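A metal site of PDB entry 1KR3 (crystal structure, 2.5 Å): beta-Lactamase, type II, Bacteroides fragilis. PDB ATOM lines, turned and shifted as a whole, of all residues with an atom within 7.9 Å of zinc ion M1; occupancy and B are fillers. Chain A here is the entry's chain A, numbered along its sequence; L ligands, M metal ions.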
ATOM      1  N   ASP A  52     -16.187   6.278  12.976  1.00  0.00           N
ATOM      2  CA  ASP A  52     -15.816   6.919  11.715  1.00  0.00           C
ATOM      3  C   ASP A  52     -14.353   6.604  11.408  1.00  0.00           C
ATOM      4  O   ASP A  52     -13.541   6.461  12.322  1.00  0.00           O
ATOM      5  CB  ASP A  52     -15.964   8.449  11.804  1.00  0.00           C
ATOM      6  CG  ASP A  52     -17.359   8.912  11.541  1.00  0.00           C
ATOM      7  OD1 ASP A  52     -18.252   8.123  11.820  1.00  0.00           O
ATOM      8  OD2 ASP A  52     -17.574  10.056  11.079  1.00  0.00           O
ATOM      9  N   ASN A  81     -20.938   6.709  11.346  1.00  0.00           N
ATOM     10  CA  ASN A  81     -22.058   7.638  11.508  1.00  0.00           C
ATOM     11  C   ASN A  81     -23.143   7.403  10.485  1.00  0.00           C
ATOM     12  O   ASN A  81     -24.345   7.458  10.814  1.00  0.00           O
ATOM     13  CB  ASN A  81     -21.606   9.078  11.414  1.00  0.00           C
ATOM     14  CG  ASN A  81     -22.708  10.058  11.779  1.00  0.00           C
ATOM     15  OD1 ASN A  81     -23.238  10.741  10.933  1.00  0.00           O
ATOM     16  ND2 ASN A  81     -23.074  10.097  13.057  1.00  0.00           N
ATOM     17  N   HIS A  82     -22.710   7.213   9.232  1.00  0.00           N
ATOM     18  CA  HIS A  82     -23.582   6.899   8.122  1.00  0.00           C
ATOM     19  C   HIS A  82     -22.752   6.314   6.956  1.00  0.00           C
ATOM     20  O   HIS A  82     -21.546   6.118   7.094  1.00  0.00           O
ATOM     21  CB  HIS A  82     -24.458   8.112   7.663  1.00  0.00           C
ATOM     22  CG  HIS A  82     -23.700   9.386   7.413  1.00  0.00           C
ATOM     23  ND1 HIS A  82     -23.146  10.159   8.393  1.00  0.00           N
ATOM     24  CD2 HIS A  82     -23.299   9.929   6.237  1.00  0.00           C
ATOM     25  CE1 HIS A  82     -22.416  11.120   7.803  1.00  0.00           C
ATOM     26  NE2 HIS A  82     -22.468  11.035   6.489  1.00  0.00           N
ATOM     27  N   TRP A  83     -23.420   6.019   5.836  1.00  0.00           N
ATOM     28  CA  TRP A  83     -22.768   5.419   4.670  1.00  0.00           C
ATOM     29  C   TRP A  83     -21.762   6.197   3.868  1.00  0.00           C
ATOM     30  O   TRP A  83     -21.217   5.630   2.932  1.00  0.00           O
ATOM     31  CB  TRP A  83     -23.803   4.908   3.666  1.00  0.00           C
ATOM     32  CG  TRP A  83     -24.590   5.978   2.928  1.00  0.00           C
ATOM     33  CD1 TRP A  83     -25.709   6.633   3.377  1.00  0.00           C
ATOM     34  CD2 TRP A  83     -24.359   6.464   1.588  1.00  0.00           C
ATOM     35  NE1 TRP A  83     -26.188   7.500   2.401  1.00  0.00           N
ATOM     36  CE2 TRP A  83     -25.364   7.412   1.297  1.00  0.00           C
ATOM     37  CE3 TRP A  83     -23.386   6.199   0.610  1.00  0.00           C
ATOM     38  CZ2 TRP A  83     -25.436   8.081   0.062  1.00  0.00           C
ATOM     39  CZ3 TRP A  83     -23.448   6.867  -0.620  1.00  0.00           C
ATOM     40  CH2 TRP A  83     -24.470   7.803  -0.878  1.00  0.00           C
ATOM     41  N   HIS A  84     -21.484   7.467   4.189  1.00  0.00           N
ATOM     42  CA  HIS A  84     -20.525   8.219   3.389  1.00  0.00           C
ATOM     43  C   HIS A  84     -19.039   7.890   3.523  1.00  0.00           C
ATOM     44  O   HIS A  84     -18.621   7.155   4.435  1.00  0.00           O
ATOM     45  CB  HIS A  84     -20.752   9.721   3.545  1.00  0.00           C
ATOM     46  CG  HIS A  84     -21.922  10.223   2.763  1.00  0.00           C
ATOM     47  ND1 HIS A  84     -22.551  11.392   3.091  1.00  0.00           N
ATOM     48  CD2 HIS A  84     -22.519   9.693   1.673  1.00  0.00           C
ATOM     49  CE1 HIS A  84     -23.516  11.547   2.200  1.00  0.00           C
ATOM     50  NE2 HIS A  84     -23.535  10.545   1.319  1.00  0.00           N
ATOM     51  N   GLY A  85     -18.266   8.403   2.567  1.00  0.00           N
ATOM     52  CA  GLY A  85     -16.833   8.170   2.522  1.00  0.00           C
ATOM     53  C   GLY A  85     -16.075   8.558   3.767  1.00  0.00           C
ATOM     54  O   GLY A  85     -15.140   7.862   4.174  1.00  0.00           O
ATOM     55  N   ASP A  86     -16.473   9.657   4.372  1.00  0.00           N
ATOM     56  CA  ASP A  86     -15.811  10.124   5.575  1.00  0.00           C
ATOM     57  C   ASP A  86     -16.324   9.459   6.875  1.00  0.00           C
ATOM     58  O   ASP A  86     -16.138   9.977   7.991  1.00  0.00           O
ATOM     59  CB  ASP A  86     -15.870  11.657   5.615  1.00  0.00           C
ATOM     60  CG  ASP A  86     -17.290  12.199   5.557  1.00  0.00           C
ATOM     61  OD1 ASP A  86     -18.068  11.737   4.697  1.00  0.00           O
ATOM     62  OD2 ASP A  86     -17.618  13.112   6.363  1.00  0.00           O
ATOM     63  N   CYS A  87     -16.933   8.283   6.730  1.00  0.00           N
ATOM     64  CA  CYS A  87     -17.419   7.525   7.867  1.00  0.00           C
ATOM     65  C   CYS A  87     -16.904   6.051   7.735  1.00  0.00           C
ATOM     66  O   CYS A  87     -16.392   5.483   8.708  1.00  0.00           O
ATOM     67  CB  CYS A  87     -18.958   7.567   7.920  1.00  0.00           C
ATOM     68  SG  CYS A  87     -19.721   9.262   7.927  1.00  0.00           S
ATOM     69  N   HIS A 145     -28.661  14.787   8.099  1.00  0.00           N
ATOM     70  CA  HIS A 145     -27.691  15.034   7.037  1.00  0.00           C
ATOM     71  C   HIS A 145     -27.858  13.975   5.967  1.00  0.00           C
ATOM     72  O   HIS A 145     -27.729  14.241   4.790  1.00  0.00           O
ATOM     73  CB  HIS A 145     -26.273  14.934   7.585  1.00  0.00           C
ATOM     74  CG  HIS A 145     -25.234  14.744   6.526  1.00  0.00           C
ATOM     75  ND1 HIS A 145     -24.749  15.782   5.761  1.00  0.00           N
ATOM     76  CD2 HIS A 145     -24.671  13.611   6.037  1.00  0.00           C
ATOM     77  CE1 HIS A 145     -23.935  15.288   4.832  1.00  0.00           C
ATOM     78  NE2 HIS A 145     -23.873  13.979   4.982  1.00  0.00           N
ATOM     79  N   ALA A 146     -28.095  12.758   6.437  1.00  0.00           N
ATOM     80  CA  ALA A 146     -28.264  11.576   5.615  1.00  0.00           C
ATOM     81  C   ALA A 146     -29.422  10.786   6.220  1.00  0.00           C
ATOM     82  O   ALA A 146     -29.683  10.916   7.407  1.00  0.00           O
ATOM     83  CB  ALA A 146     -26.960  10.753   5.665  1.00  0.00           C
ATOM     84  N   ASP A 148     -29.700   7.685   7.025  1.00  0.00           N
ATOM     85  CA  ASP A 148     -29.246   6.683   7.987  1.00  0.00           C
ATOM     86  C   ASP A 148     -28.461   7.124   9.206  1.00  0.00           C
ATOM     87  O   ASP A 148     -28.139   6.298  10.050  1.00  0.00           O
ATOM     88  CB  ASP A 148     -28.426   5.583   7.238  1.00  0.00           C
ATOM     89  CG  ASP A 148     -27.148   6.115   6.550  1.00  0.00           C
ATOM     90  OD1 ASP A 148     -26.073   5.460   6.737  1.00  0.00           O
ATOM     91  OD2 ASP A 148     -27.195   7.132   5.808  1.00  0.00           O
ATOM     92  N   ASN A 149     -28.163   8.417   9.299  1.00  0.00           N
ATOM     93  CA  ASN A 149     -27.357   8.925  10.413  1.00  0.00           C
ATOM     94  C   ASN A 149     -27.772   8.710  11.879  1.00  0.00           C
ATOM     95  O   ASN A 149     -28.910   8.946  12.283  1.00  0.00           O
ATOM     96  CB  ASN A 149     -27.032  10.433  10.175  1.00  0.00           C
ATOM     97  CG  ASN A 149     -28.272  11.346  10.190  1.00  0.00           C
ATOM     98  OD1 ASN A 149     -28.178  12.510   9.781  1.00  0.00           O
ATOM     99  ND2 ASN A 149     -29.396  10.851  10.673  1.00  0.00           N
ATOM    100  N   GLY A 163     -21.737  13.661  14.614  1.00  0.00           N
ATOM    101  CA  GLY A 163     -21.607  13.435  13.198  1.00  0.00           C
ATOM    102  C   GLY A 163     -22.014  14.671  12.404  1.00  0.00           C
ATOM    103  O   GLY A 163     -22.195  15.756  12.947  1.00  0.00           O
ATOM    104  N   CYS A 164     -22.204  14.473  11.110  1.00  0.00           N
ATOM    105  CA  CYS A 164     -22.561  15.547  10.211  1.00  0.00           C
ATOM    106  C   CYS A 164     -23.992  16.057  10.312  1.00  0.00           C
ATOM    107  O   CYS A 164     -24.365  16.954   9.563  1.00  0.00           O
ATOM    108  CB  CYS A 164     -22.239  15.121   8.781  1.00  0.00           C
ATOM    109  SG  CYS A 164     -20.559  14.465   8.739  1.00  0.00           S
ATOM    110  N   MET A 165     -24.794  15.528  11.213  1.00  0.00           N
ATOM    111  CA  MET A 165     -26.128  16.124  11.334  1.00  0.00           C
ATOM    112  C   MET A 165     -25.886  17.395  12.131  1.00  0.00           C
ATOM    113  O   MET A 165     -26.703  18.291  12.114  1.00  0.00           O
ATOM    114  CB  MET A 165     -27.170  15.236  12.079  1.00  0.00           C
ATOM    115  CG  MET A 165     -27.140  15.272  13.598  1.00  0.00           C
ATOM    116  SD  MET A 165     -28.501  14.292  14.280  1.00  0.00           S
ATOM    117  CE  MET A 165     -28.155  12.535  13.643  1.00  0.00           C
ATOM    118  N   ASN A 176     -23.303  20.223   2.009  1.00  0.00           N
ATOM    119  CA  ASN A 176     -23.645  19.009   1.242  1.00  0.00           C
ATOM    120  C   ASN A 176     -24.964  18.273   1.540  1.00  0.00           C
ATOM    121  O   ASN A 176     -24.968  17.264   2.273  1.00  0.00           O
ATOM    122  CB  ASN A 176     -22.466  18.025   1.395  1.00  0.00           C
ATOM    123  CG  ASN A 176     -22.655  16.758   0.602  1.00  0.00           C
ATOM    124  OD1 ASN A 176     -22.830  16.802  -0.620  1.00  0.00           O
ATOM    125  ND2 ASN A 176     -22.602  15.621   1.292  1.00  0.00           N
ATOM    126  N   ASP A 179     -27.863  13.765   0.015  1.00  0.00           N
ATOM    127  CA  ASP A 179     -28.520  12.573   0.557  1.00  0.00           C
ATOM    128  C   ASP A 179     -29.292  13.014   1.793  1.00  0.00           C
ATOM    129  O   ASP A 179     -29.863  12.184   2.510  1.00  0.00           O
ATOM    130  CB  ASP A 179     -27.484  11.541   0.985  1.00  0.00           C
ATOM    131  CG  ASP A 179     -26.623  11.059  -0.163  1.00  0.00           C
ATOM    132  OD1 ASP A 179     -27.119  10.230  -0.923  1.00  0.00           O
ATOM    133  OD2 ASP A 179     -25.469  11.522  -0.314  1.00  0.00           O
ATOM    134  N   HIS A 206     -17.665  17.830  11.052  1.00  0.00           N
ATOM    135  CA  HIS A 206     -16.620  18.724  10.488  1.00  0.00           C
ATOM    136  C   HIS A 206     -16.549  19.962  11.340  1.00  0.00           C
ATOM    137  O   HIS A 206     -17.578  20.510  11.725  1.00  0.00           O
ATOM    138  CB  HIS A 206     -16.954  19.103   9.040  1.00  0.00           C
ATOM    139  CG  HIS A 206     -16.967  17.923   8.120  1.00  0.00           C
ATOM    140  ND1 HIS A 206     -15.818  17.392   7.555  1.00  0.00           N
ATOM    141  CD2 HIS A 206     -17.968  17.085   7.775  1.00  0.00           C
ATOM    142  CE1 HIS A 206     -16.115  16.293   6.899  1.00  0.00           C
ATOM    143  NE2 HIS A 206     -17.417  16.079   7.022  1.00  0.00           N
HETATM  144  C1  LIG L   1     -18.573  16.855   2.247  1.00  0.00           C
HETATM  145  C2  LIG L   1     -17.993  18.105   1.994  1.00  0.00           C
HETATM  146  C3  LIG L   1     -18.076  19.089   2.971  1.00  0.00           C
HETATM  147  C4  LIG L   1     -18.893  18.898   4.094  1.00  0.00           C
HETATM  148  C5  LIG L   1     -19.811  17.816   4.100  1.00  0.00           C
HETATM  149  C6  LIG L   1     -19.562  16.728   3.226  1.00  0.00           C
HETATM  150  O1  LIG L   1     -17.335  20.250   2.836  1.00  0.00           O
HETATM  151  C7  LIG L   1     -17.367  21.260   3.778  1.00  0.00           C
HETATM  152  C8  LIG L   1     -18.010  21.128   4.961  1.00  0.00           C
HETATM  153  C9  LIG L   1     -18.752  19.830   5.222  1.00  0.00           C
HETATM  154  C10 LIG L   1     -16.634  22.514   3.390  1.00  0.00           C
HETATM  155  C11 LIG L   1     -17.228  23.744   4.122  1.00  0.00           C
HETATM  156  O2  LIG L   1     -17.383  23.478   5.521  1.00  0.00           O
HETATM  157  C12 LIG L   1     -18.003  22.273   5.983  1.00  0.00           C
HETATM  158  O3  LIG L   1     -20.235  15.511   3.257  1.00  0.00           O
HETATM  159  O4  LIG L   1     -18.185  15.718   1.564  1.00  0.00           O
HETATM  160  C13 LIG L   1     -21.008  17.810   4.974  1.00  0.00           C
HETATM  161  O5  LIG L   1     -20.837  17.235   6.175  1.00  0.00           O
HETATM  162  O6  LIG L   1     -19.285  22.527   6.557  1.00  0.00           O
HETATM  163  C14 LIG L   1     -20.335  23.089   5.785  1.00  0.00           C
HETATM  164  C15 LIG L   1     -16.375  25.011   3.952  1.00  0.00           C
HETATM  165  O7  LIG L   1     -22.054  18.337   4.637  1.00  0.00           O
HETATM  166  O8  LIG L   1     -19.182  19.620   6.342  1.00  0.00           O
HETATM  167 ZN    ZN M   1     -21.955  12.540   5.075  1.00  0.00          ZN
HETATM  168 ZN    ZN M   2     -20.054  14.788   6.770  1.00  0.00          ZN
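O3 of the ligand is in hydrogen-bond range of ND2 of Asn 176. An oxygen (O5) of the ligand sits close to the side-chain sulfur (SG) of Cys 164, at 3.8 Å. O7 of the ligand sits close to N of Asn 176 (3.5 Å).
The side-chain carboxylate (OD2) of Asp 86 is in hydrogen-bond range of a ring nitrogen (NE2) of His 206 (3.0 Å). OD1 of Asn 81 lies within hydrogen-bond range of ND1 of His 82 (2.6 Å). The backbone NH (N) of His 145 is in hydrogen-bond range of the side-chain amide oxygen (OD1) of Asn 149 (2.9 Å). A ring nitrogen (ND1) of His 82 lies close to the side-chain sulfur (SG) of Cys 87 (3.6 Å). NE2 of His 84 lies within hydrogen-bond range of OD2 of Asp 179 (2.7 Å).
Residues that only touch zinc ion M1: Asp 86 (3.99 Å). Of the 18 residues printed, 4 come within 4 Å of zinc ion M1. The nearest printed residue that does not touch zinc ion M1 is Cys 164 (4.4 Å).
Zinc ion M1 is bound by a ring nitrogen (NE2) of His 82 (2.1 Å), a ring nitrogen (ND1) of His 84 (2.4 Å) and a ring nitrogen (NE2) of His 145 (2.4 Å). Zinc ion M1 has three donor atoms within binding distance.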
